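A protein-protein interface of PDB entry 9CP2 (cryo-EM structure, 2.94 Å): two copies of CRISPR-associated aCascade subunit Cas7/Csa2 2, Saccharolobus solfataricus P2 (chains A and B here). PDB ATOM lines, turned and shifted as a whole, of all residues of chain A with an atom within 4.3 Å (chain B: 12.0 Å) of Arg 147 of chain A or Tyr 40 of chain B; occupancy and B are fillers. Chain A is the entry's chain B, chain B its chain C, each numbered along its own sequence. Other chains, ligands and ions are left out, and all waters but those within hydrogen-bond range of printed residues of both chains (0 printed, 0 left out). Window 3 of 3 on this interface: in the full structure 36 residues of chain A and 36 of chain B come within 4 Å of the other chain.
Hydrophobic or aromatic side chains of chain A within 4 Å of the printed part of chain B: Leu 183.
Printed residues of chain B that touch a printed residue of chain A: Val 33, Lys 35 and Tyr 40.
Among the printed residues, 5 pairs touch across the chains.
Among the printed residues, no Asp or Glu carboxylate lies within 4 Å of a Lys or Arg side-chain nitrogen of the other chain.
Arg 147 of chain A touches Tyr 40 of chain B (NH2 to CD1, 3.1 Å).
Val 33 of chain B touches Pro 152 of chain A.
Tyr 40 of chain B touches Leu 183 of chain A.
O of Glu 297 of chain A touches NZ of Lys 35 of chain B, at 3.5 Å.
O of Leu 183 of chain A lies within hydrogen-bond range of N of Ala 145 of chain A, 3.0 Å away.
5 positions are printed for both chains.
Of the 5 pairs that touch across the chains among the printed residues, none has its exchanged pair printed and touching as well.
The side-chain carboxylate of Glu 297 of chain A is in hydrogen-bond range of the side-chain hydroxyl of Tyr 40 of chain B (3.0 Å).
No residue of chain B comes within 4 Å of Ala 145 of chain A.
No residue of chain B comes within 4 Å of Leu 146 of chain A.
Arg 147 of chain A touches one residue of chain B.
No residue of chain B comes within 4 Å of Gly 148 of chain A.
Printed residues of chain B within 4 Å of Pro 152 of chain A: Val 33.
Leu 183 of chain A touches just one residue of chain B: Tyr 40 (3.6 Å).
His 265 of chain A touches none of the printed residues of chain B.
No residue of chain B comes within 4 Å of Asp 267 of chain A.
Of the printed residues of chain A, Val 33 of chain B touches Pro 152 (3.7 Å).
Printed residues of chain A within 4 Å of Lys 35 of chain B: Glu 297 (3.5 Å).
Tyr 40 of chain B touches three residues of chain A.
Val 42 of chain B touches none of the printed residues of chain A.
Asp 266 of chain B touches none of the printed residues of chain A.
The nearest residue of chain B that does not touch Arg 147 of chain A is Gly 39 of chain B (5.1 Å).
The nearest residue of chain A that does not touch Tyr 40 of chain B is Pro 152 of chain A (4.1 Å).
The nearest printed residue of chain A that does not touch Lys 35 of chain B is Leu 183 of chain A (6.9 Å).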
ATOM      1  N   ALA A 145      13.622  13.517   1.312  1.00  0.00           N
ATOM      2  CA  ALA A 145      14.596  13.840   0.277  1.00  0.00           C
ATOM      3  C   ALA A 145      15.632  12.733   0.147  1.00  0.00           C
ATOM      4  O   ALA A 145      16.322  12.393   1.112  1.00  0.00           O
ATOM      5  CB  ALA A 145      15.279  15.168   0.597  1.00  0.00           C
ATOM      6  N   LEU A 146      15.747  12.179  -1.058  1.00  0.00           N
ATOM      7  CA  LEU A 146      16.689  11.095  -1.333  1.00  0.00           C
ATOM      8  C   LEU A 146      18.061  11.665  -1.694  1.00  0.00           C
ATOM      9  O   LEU A 146      18.566  11.523  -2.805  1.00  0.00           O
ATOM     10  CB  LEU A 146      16.149  10.199  -2.441  1.00  0.00           C
ATOM     11  CG  LEU A 146      14.771   9.589  -2.197  1.00  0.00           C
ATOM     12  CD1 LEU A 146      14.298   8.840  -3.428  1.00  0.00           C
ATOM     13  CD2 LEU A 146      14.802   8.674  -0.990  1.00  0.00           C
ATOM     14  N   ARG A 147      18.660  12.327  -0.712  1.00  0.00           N
ATOM     15  CA  ARG A 147      19.929  13.014  -0.886  1.00  0.00           C
ATOM     16  C   ARG A 147      21.045  12.215  -0.228  1.00  0.00           C
ATOM     17  O   ARG A 147      20.886  11.711   0.888  1.00  0.00           O
ATOM     18  CB  ARG A 147      19.868  14.415  -0.279  1.00  0.00           C
ATOM     19  CG  ARG A 147      21.048  15.301  -0.621  1.00  0.00           C
ATOM     20  CD  ARG A 147      20.960  16.608   0.140  1.00  0.00           C
ATOM     21  NE  ARG A 147      20.352  16.404   1.449  1.00  0.00           N
ATOM     22  CZ  ARG A 147      21.026  16.060   2.536  1.00  0.00           C
ATOM     23  NH1 ARG A 147      22.341  15.918   2.518  1.00  0.00           N
ATOM     24  NH2 ARG A 147      20.365  15.851   3.670  1.00  0.00           N
ATOM     25  N   GLY A 148      22.173  12.101  -0.925  1.00  0.00           N
ATOM     26  CA  GLY A 148      23.310  11.404  -0.359  1.00  0.00           C
ATOM     27  C   GLY A 148      23.059   9.912  -0.215  1.00  0.00           C
ATOM     28  O   GLY A 148      22.299   9.299  -0.969  1.00  0.00           O
ATOM     29  N   ASP A 149      23.714   9.319   0.788  1.00  0.00           N
ATOM     30  CA  ASP A 149      23.627   7.887   1.032  1.00  0.00           C
ATOM     31  C   ASP A 149      22.695   7.510   2.173  1.00  0.00           C
ATOM     32  O   ASP A 149      22.216   6.373   2.201  1.00  0.00           O
ATOM     33  CB  ASP A 149      25.021   7.314   1.332  1.00  0.00           C
ATOM     34  CG  ASP A 149      25.987   7.502   0.181  1.00  0.00           C
ATOM     35  OD1 ASP A 149      25.611   8.159  -0.812  1.00  0.00           O
ATOM     36  OD2 ASP A 149      27.125   6.996   0.273  1.00  0.00           O
ATOM     37  N   GLU A 150      22.427   8.420   3.103  1.00  0.00           N
ATOM     38  CA  GLU A 150      21.581   8.149   4.257  1.00  0.00           C
ATOM     39  C   GLU A 150      20.301   8.966   4.156  1.00  0.00           C
ATOM     40  O   GLU A 150      20.352  10.187   3.981  1.00  0.00           O
ATOM     41  CB  GLU A 150      22.311   8.475   5.560  1.00  0.00           C
ATOM     42  CG  GLU A 150      23.752   8.002   5.597  1.00  0.00           C
ATOM     43  CD  GLU A 150      24.391   8.198   6.956  1.00  0.00           C
ATOM     44  OE1 GLU A 150      23.727   8.765   7.849  1.00  0.00           O
ATOM     45  OE2 GLU A 150      25.555   7.785   7.131  1.00  0.00           O
ATOM     46  N   PRO A 152      17.348  10.987   5.497  1.00  0.00           N
ATOM     47  CA  PRO A 152      17.160  11.756   6.745  1.00  0.00           C
ATOM     48  C   PRO A 152      15.731  11.677   7.270  1.00  0.00           C
ATOM     49  O   PRO A 152      14.990  12.661   7.337  1.00  0.00           O
ATOM     50  CB  PRO A 152      17.557  13.170   6.315  1.00  0.00           C
ATOM     51  CG  PRO A 152      17.151  13.239   4.881  1.00  0.00           C
ATOM     52  CD  PRO A 152      17.261  11.846   4.304  1.00  0.00           C
ATOM     53  N   LEU A 183      12.182  15.000   6.332  1.00  0.00           N
ATOM     54  CA  LEU A 183      12.422  16.174   5.499  1.00  0.00           C
ATOM     55  C   LEU A 183      11.663  15.924   4.199  1.00  0.00           C
ATOM     56  O   LEU A 183      12.193  15.341   3.252  1.00  0.00           O
ATOM     57  CB  LEU A 183      13.913  16.393   5.263  1.00  0.00           C
ATOM     58  CG  LEU A 183      14.309  17.471   4.253  1.00  0.00           C
ATOM     59  CD1 LEU A 183      14.099  18.859   4.832  1.00  0.00           C
ATOM     60  CD2 LEU A 183      15.751  17.290   3.816  1.00  0.00           C
ATOM     61  N   HIS A 265      15.293  16.870  -4.635  1.00  0.00           N
ATOM     62  CA  HIS A 265      16.118  15.844  -4.007  1.00  0.00           C
ATOM     63  C   HIS A 265      17.555  16.322  -3.812  1.00  0.00           C
ATOM     64  O   HIS A 265      18.053  16.367  -2.683  1.00  0.00           O
ATOM     65  CB  HIS A 265      16.076  14.559  -4.840  1.00  0.00           C
ATOM     66  CG  HIS A 265      14.744  13.881  -4.825  1.00  0.00           C
ATOM     67  ND1 HIS A 265      14.412  12.869  -5.700  1.00  0.00           N
ATOM     68  CD2 HIS A 265      13.655  14.073  -4.044  1.00  0.00           C
ATOM     69  CE1 HIS A 265      13.178  12.466  -5.457  1.00  0.00           C
ATOM     70  NE2 HIS A 265      12.697  13.180  -4.455  1.00  0.00           N
ATOM     71  N   ASP A 267      20.759  18.934  -3.634  1.00  0.00           N
ATOM     72  CA  ASP A 267      20.928  20.275  -3.087  1.00  0.00           C
ATOM     73  C   ASP A 267      20.863  21.351  -4.162  1.00  0.00           C
ATOM     74  O   ASP A 267      20.625  22.519  -3.836  1.00  0.00           O
ATOM     75  CB  ASP A 267      22.255  20.376  -2.334  1.00  0.00           C
ATOM     76  CG  ASP A 267      22.158  19.868  -0.909  1.00  0.00           C
ATOM     77  OD1 ASP A 267      21.077  20.002  -0.299  1.00  0.00           O
ATOM     78  OD2 ASP A 267      23.166  19.341  -0.395  1.00  0.00           O
ATOM     79  N   GLU A 297      17.343  28.049   3.563  1.00  0.00           N
ATOM     80  CA  GLU A 297      18.423  27.182   4.013  1.00  0.00           C
ATOM     81  C   GLU A 297      19.792  27.598   3.495  1.00  0.00           C
ATOM     82  O   GLU A 297      20.804  27.127   4.025  1.00  0.00           O
ATOM     83  CB  GLU A 297      18.141  25.733   3.595  1.00  0.00           C
ATOM     84  CG  GLU A 297      17.821  25.565   2.123  1.00  0.00           C
ATOM     85  CD  GLU A 297      17.358  24.163   1.786  1.00  0.00           C
ATOM     86  OE1 GLU A 297      17.157  23.362   2.721  1.00  0.00           O
ATOM     87  OE2 GLU A 297      17.192  23.861   0.587  1.00  0.00           O
ATOM     88  N   PRO B  31      12.853  10.570  18.081  1.00  0.00           N
ATOM     89  CA  PRO B  31      13.831  11.013  17.083  1.00  0.00           C
ATOM     90  C   PRO B  31      13.415  12.315  16.419  1.00  0.00           C
ATOM     91  O   PRO B  31      12.239  12.545  16.129  1.00  0.00           O
ATOM     92  CB  PRO B  31      13.847   9.863  16.066  1.00  0.00           C
ATOM     93  CG  PRO B  31      12.969   8.784  16.646  1.00  0.00           C
ATOM     94  CD  PRO B  31      12.028   9.469  17.567  1.00  0.00           C
ATOM     95  N   VAL B  32      14.405  13.164  16.170  1.00  0.00           N
ATOM     96  CA  VAL B  32      14.208  14.447  15.513  1.00  0.00           C
ATOM     97  C   VAL B  32      15.244  14.603  14.409  1.00  0.00           C
ATOM     98  O   VAL B  32      16.375  14.114  14.510  1.00  0.00           O
ATOM     99  CB  VAL B  32      14.289  15.632  16.503  1.00  0.00           C
ATOM    100  CG1 VAL B  32      13.275  15.466  17.620  1.00  0.00           C
ATOM    101  CG2 VAL B  32      15.688  15.760  17.074  1.00  0.00           C
ATOM    102  N   VAL B  33      14.839  15.289  13.341  1.00  0.00           N
ATOM    103  CA  VAL B  33      15.695  15.590  12.200  1.00  0.00           C
ATOM    104  C   VAL B  33      16.135  17.041  12.314  1.00  0.00           C
ATOM    105  O   VAL B  33      15.298  17.942  12.445  1.00  0.00           O
ATOM    106  CB  VAL B  33      14.967  15.340  10.868  1.00  0.00           C
ATOM    107  CG1 VAL B  33      15.902  15.599   9.702  1.00  0.00           C
ATOM    108  CG2 VAL B  33      14.418  13.924  10.821  1.00  0.00           C
ATOM    109  N   LEU B  34      17.443  17.267  12.268  1.00  0.00           N
ATOM    110  CA  LEU B  34      18.009  18.588  12.496  1.00  0.00           C
ATOM    111  C   LEU B  34      18.953  18.944  11.358  1.00  0.00           C
ATOM    112  O   LEU B  34      19.559  18.067  10.739  1.00  0.00           O
ATOM    113  CB  LEU B  34      18.733  18.638  13.850  1.00  0.00           C
ATOM    114  CG  LEU B  34      19.265  19.959  14.405  1.00  0.00           C
ATOM    115  CD1 LEU B  34      19.306  19.876  15.906  1.00  0.00           C
ATOM    116  CD2 LEU B  34      20.654  20.235  13.897  1.00  0.00           C
ATOM    117  N   LYS B  35      19.069  20.239  11.079  1.00  0.00           N
ATOM    118  CA  LYS B  35      19.937  20.732  10.017  1.00  0.00           C
ATOM    119  C   LYS B  35      21.133  21.454  10.626  1.00  0.00           C
ATOM    120  O   LYS B  35      20.968  22.455  11.331  1.00  0.00           O
ATOM    121  CB  LYS B  35      19.172  21.657   9.072  1.00  0.00           C
ATOM    122  CG  LYS B  35      19.997  22.137   7.892  1.00  0.00           C
ATOM    123  CD  LYS B  35      19.184  23.006   6.951  1.00  0.00           C
ATOM    124  CE  LYS B  35      20.008  23.391   5.737  1.00  0.00           C
ATOM    125  NZ  LYS B  35      21.127  24.298   6.108  1.00  0.00           N
ATOM    126  N   THR B  36      22.329  20.943  10.356  1.00  0.00           N
ATOM    127  CA  THR B  36      23.584  21.553  10.764  1.00  0.00           C
ATOM    128  C   THR B  36      24.259  22.190   9.558  1.00  0.00           C
ATOM    129  O   THR B  36      23.721  22.206   8.449  1.00  0.00           O
ATOM    130  CB  THR B  36      24.526  20.523  11.400  1.00  0.00           C
ATOM    131  OG1 THR B  36      24.734  19.436  10.490  1.00  0.00           O
ATOM    132  CG2 THR B  36      23.961  19.994  12.702  1.00  0.00           C
ATOM    133  N   SER B  37      25.461  22.723   9.793  1.00  0.00           N
ATOM    134  CA  SER B  37      26.260  23.239   8.686  1.00  0.00           C
ATOM    135  C   SER B  37      26.679  22.124   7.739  1.00  0.00           C
ATOM    136  O   SER B  37      26.746  22.334   6.523  1.00  0.00           O
ATOM    137  CB  SER B  37      27.489  23.974   9.220  1.00  0.00           C
ATOM    138  OG  SER B  37      28.437  23.069   9.756  1.00  0.00           O
ATOM    139  N   THR B  38      26.958  20.935   8.272  1.00  0.00           N
ATOM    140  CA  THR B  38      27.421  19.815   7.462  1.00  0.00           C
ATOM    141  C   THR B  38      26.294  19.082   6.750  1.00  0.00           C
ATOM    142  O   THR B  38      26.574  18.269   5.864  1.00  0.00           O
ATOM    143  CB  THR B  38      28.193  18.821   8.331  1.00  0.00           C
ATOM    144  OG1 THR B  38      27.296  18.202   9.261  1.00  0.00           O
ATOM    145  CG2 THR B  38      29.295  19.531   9.101  1.00  0.00           C
ATOM    146  N   GLY B  39      25.039  19.337   7.109  1.00  0.00           N
ATOM    147  CA  GLY B  39      23.931  18.674   6.452  1.00  0.00           C
ATOM    148  C   GLY B  39      22.753  18.398   7.362  1.00  0.00           C
ATOM    149  O   GLY B  39      22.326  19.274   8.119  1.00  0.00           O
ATOM    150  N   TYR B  40      22.223  17.181   7.298  1.00  0.00           N
ATOM    151  CA  TYR B  40      21.050  16.791   8.065  1.00  0.00           C
ATOM    152  C   TYR B  40      21.383  15.575   8.915  1.00  0.00           C
ATOM    153  O   TYR B  40      22.032  14.636   8.446  1.00  0.00           O
ATOM    154  CB  TYR B  40      19.863  16.483   7.145  1.00  0.00           C
ATOM    155  CG  TYR B  40      19.274  17.704   6.472  1.00  0.00           C
ATOM    156  CD1 TYR B  40      19.969  18.376   5.478  1.00  0.00           C
ATOM    157  CD2 TYR B  40      18.019  18.176   6.824  1.00  0.00           C
ATOM    158  CE1 TYR B  40      19.437  19.487   4.860  1.00  0.00           C
ATOM    159  CE2 TYR B  40      17.478  19.289   6.210  1.00  0.00           C
ATOM    160  CZ  TYR B  40      18.192  19.938   5.228  1.00  0.00           C
ATOM    161  OH  TYR B  40      17.664  21.046   4.611  1.00  0.00           O
ATOM    162  N   LEU B  41      20.930  15.596  10.167  1.00  0.00           N
ATOM    163  CA  LEU B  41      21.241  14.555  11.133  1.00  0.00           C
ATOM    164  C   LEU B  41      19.971  14.107  11.840  1.00  0.00           C
ATOM    165  O   LEU B  41      18.952  14.804  11.841  1.00  0.00           O
ATOM    166  CB  LEU B  41      22.264  15.036  12.169  1.00  0.00           C
ATOM    167  CG  LEU B  41      23.564  15.633  11.632  1.00  0.00           C
ATOM    168  CD1 LEU B  41      24.392  16.214  12.765  1.00  0.00           C
ATOM    169  CD2 LEU B  41      24.354  14.593  10.865  1.00  0.00           C
ATOM    170  N   VAL B  42      20.052  12.928  12.452  1.00  0.00           N
ATOM    171  CA  VAL B  42      18.967  12.343  13.230  1.00  0.00           C
ATOM    172  C   VAL B  42      19.457  12.161  14.659  1.00  0.00           C
ATOM    173  O   VAL B  42      20.556  11.637  14.878  1.00  0.00           O
ATOM    174  CB  VAL B  42      18.504  11.002  12.634  1.00  0.00           C
ATOM    175  CG1 VAL B  42      17.388  10.405  13.469  1.00  0.00           C
ATOM    176  CG2 VAL B  42      18.058  11.191  11.196  1.00  0.00           C
ATOM    177  N   ARG B  43      18.652  12.594  15.625  1.00  0.00           N
ATOM    178  CA  ARG B  43      19.028  12.506  17.029  1.00  0.00           C
ATOM    179  C   ARG B  43      17.863  11.983  17.855  1.00  0.00           C
ATOM    180  O   ARG B  43      16.705  12.058  17.447  1.00  0.00           O
ATOM    181  CB  ARG B  43      19.482  13.865  17.573  1.00  0.00           C
ATOM    182  CG  ARG B  43      20.800  14.343  17.005  1.00  0.00           C
ATOM    183  CD  ARG B  43      21.964  13.659  17.695  1.00  0.00           C
ATOM    184  NE  ARG B  43      23.225  13.891  17.002  1.00  0.00           N
ATOM    185  CZ  ARG B  43      23.914  15.022  17.055  1.00  0.00           C
ATOM    186  NH1 ARG B  43      23.494  16.056  17.767  1.00  0.00           N
ATOM    187  NH2 ARG B  43      25.054  15.119  16.377  1.00  0.00           N
ATOM    188  N   TYR B  44      18.184  11.441  19.027  1.00  0.00           N
ATOM    189  CA  TYR B  44      17.188  10.960  19.977  1.00  0.00           C
ATOM    190  C   TYR B  44      17.204  11.878  21.190  1.00  0.00           C
ATOM    191  O   TYR B  44      18.227  11.990  21.873  1.00  0.00           O
ATOM    192  CB  TYR B  44      17.474   9.517  20.385  1.00  0.00           C
ATOM    193  CG  TYR B  44      17.033   8.495  19.364  1.00  0.00           C
ATOM    194  CD1 TYR B  44      17.771   8.274  18.210  1.00  0.00           C
ATOM    195  CD2 TYR B  44      15.881   7.749  19.555  1.00  0.00           C
ATOM    196  CE1 TYR B  44      17.371   7.340  17.275  1.00  0.00           C
ATOM    197  CE2 TYR B  44      15.473   6.815  18.627  1.00  0.00           C
ATOM    198  CZ  TYR B  44      16.221   6.614  17.490  1.00  0.00           C
ATOM    199  OH  TYR B  44      15.815   5.682  16.564  1.00  0.00           O
ATOM    200  N   LEU B 146      14.992  23.377  18.305  1.00  0.00           N
ATOM    201  CA  LEU B 146      16.002  22.940  17.342  1.00  0.00           C
ATOM    202  C   LEU B 146      16.754  24.148  16.784  1.00  0.00           C
ATOM    203  O   LEU B 146      16.625  24.529  15.623  1.00  0.00           O
ATOM    204  CB  LEU B 146      15.357  22.120  16.232  1.00  0.00           C
ATOM    205  CG  LEU B 146      14.550  20.910  16.697  1.00  0.00           C
ATOM    206  CD1 LEU B 146      14.008  20.156  15.504  1.00  0.00           C
ATOM    207  CD2 LEU B 146      15.399  20.005  17.565  1.00  0.00           C
ATOM    208  N   GLY B 148      20.402  26.159  16.151  1.00  0.00           N
ATOM    209  CA  GLY B 148      21.822  25.932  15.963  1.00  0.00           C
ATOM    210  C   GLY B 148      22.133  24.485  15.618  1.00  0.00           C
ATOM    211  O   GLY B 148      21.314  23.757  15.051  1.00  0.00           O
ATOM    212  N   ASP B 149      23.348  24.063  15.975  1.00  0.00           N
ATOM    213  CA  ASP B 149      23.811  22.712  15.695  1.00  0.00           C
ATOM    214  C   ASP B 149      23.813  21.795  16.909  1.00  0.00           C
ATOM    215  O   ASP B 149      23.848  20.574  16.735  1.00  0.00           O
ATOM    216  CB  ASP B 149      25.226  22.745  15.101  1.00  0.00           C
ATOM    217  CG  ASP B 149      25.270  23.401  13.737  1.00  0.00           C
ATOM    218  OD1 ASP B 149      24.229  23.934  13.298  1.00  0.00           O
ATOM    219  OD2 ASP B 149      26.345  23.385  13.102  1.00  0.00           O
ATOM    220  N   GLU B 150      23.782  22.343  18.120  1.00  0.00           N
ATOM    221  CA  GLU B 150      23.765  21.552  19.342  1.00  0.00           C
ATOM    222  C   GLU B 150      22.411  21.698  20.020  1.00  0.00           C
ATOM    223  O   GLU B 150      21.983  22.816  20.326  1.00  0.00           O
ATOM    224  CB  GLU B 150      24.880  21.988  20.295  1.00  0.00           C
ATOM    225  CG  GLU B 150      26.206  22.258  19.612  1.00  0.00           C
ATOM    226  CD  GLU B 150      27.323  22.518  20.600  1.00  0.00           C
ATOM    227  OE1 GLU B 150      27.047  22.541  21.817  1.00  0.00           O
ATOM    228  OE2 GLU B 150      28.477  22.700  20.159  1.00  0.00           O
ATOM    229  N   ILE B 151      21.744  20.573  20.252  1.00  0.00           N
ATOM    230  CA  ILE B 151      20.438  20.570  20.903  1.00  0.00           C
ATOM    231  C   ILE B 151      20.625  20.930  22.372  1.00  0.00           C
ATOM    232  O   ILE B 151      21.479  20.342  23.049  1.00  0.00           O
ATOM    233  CB  ILE B 151      19.743  19.209  20.747  1.00  0.00           C
ATOM    234  CG1 ILE B 151      19.678  18.823  19.271  1.00  0.00           C
ATOM    235  CG2 ILE B 151      18.346  19.257  21.335  1.00  0.00           C
ATOM    236  CD1 ILE B 151      19.107  17.454  19.022  1.00  0.00           C
ATOM    237  N   HIS B 265      11.422  27.685  17.209  1.00  0.00           N
ATOM    238  CA  HIS B 265      12.725  27.088  16.946  1.00  0.00           C
ATOM    239  C   HIS B 265      13.791  28.160  16.751  1.00  0.00           C
ATOM    240  O   HIS B 265      14.781  28.207  17.488  1.00  0.00           O
ATOM    241  CB  HIS B 265      12.648  26.182  15.713  1.00  0.00           C
ATOM    242  CG  HIS B 265      11.857  24.931  15.929  1.00  0.00           C
ATOM    243  ND1 HIS B 265      11.430  24.134  14.890  1.00  0.00           N
ATOM    244  CD2 HIS B 265      11.419  24.337  17.064  1.00  0.00           C
ATOM    245  CE1 HIS B 265      10.765  23.101  15.376  1.00  0.00           C
ATOM    246  NE2 HIS B 265      10.741  23.201  16.692  1.00  0.00           N
ATOM    247  N   ASP B 266      13.593  29.029  15.765  1.00  0.00           N
ATOM    248  CA  ASP B 266      14.556  30.070  15.455  1.00  0.00           C
ATOM    249  C   ASP B 266      14.446  31.219  16.451  1.00  0.00           C
ATOM    250  O   ASP B 266      13.380  31.501  17.005  1.00  0.00           O
ATOM    251  CB  ASP B 266      14.343  30.582  14.033  1.00  0.00           C
ATOM    252  CG  ASP B 266      14.299  29.464  13.014  1.00  0.00           C
ATOM    253  OD1 ASP B 266      15.015  28.459  13.201  1.00  0.00           O
ATOM    254  OD2 ASP B 266      13.548  29.586  12.023  1.00  0.00           O
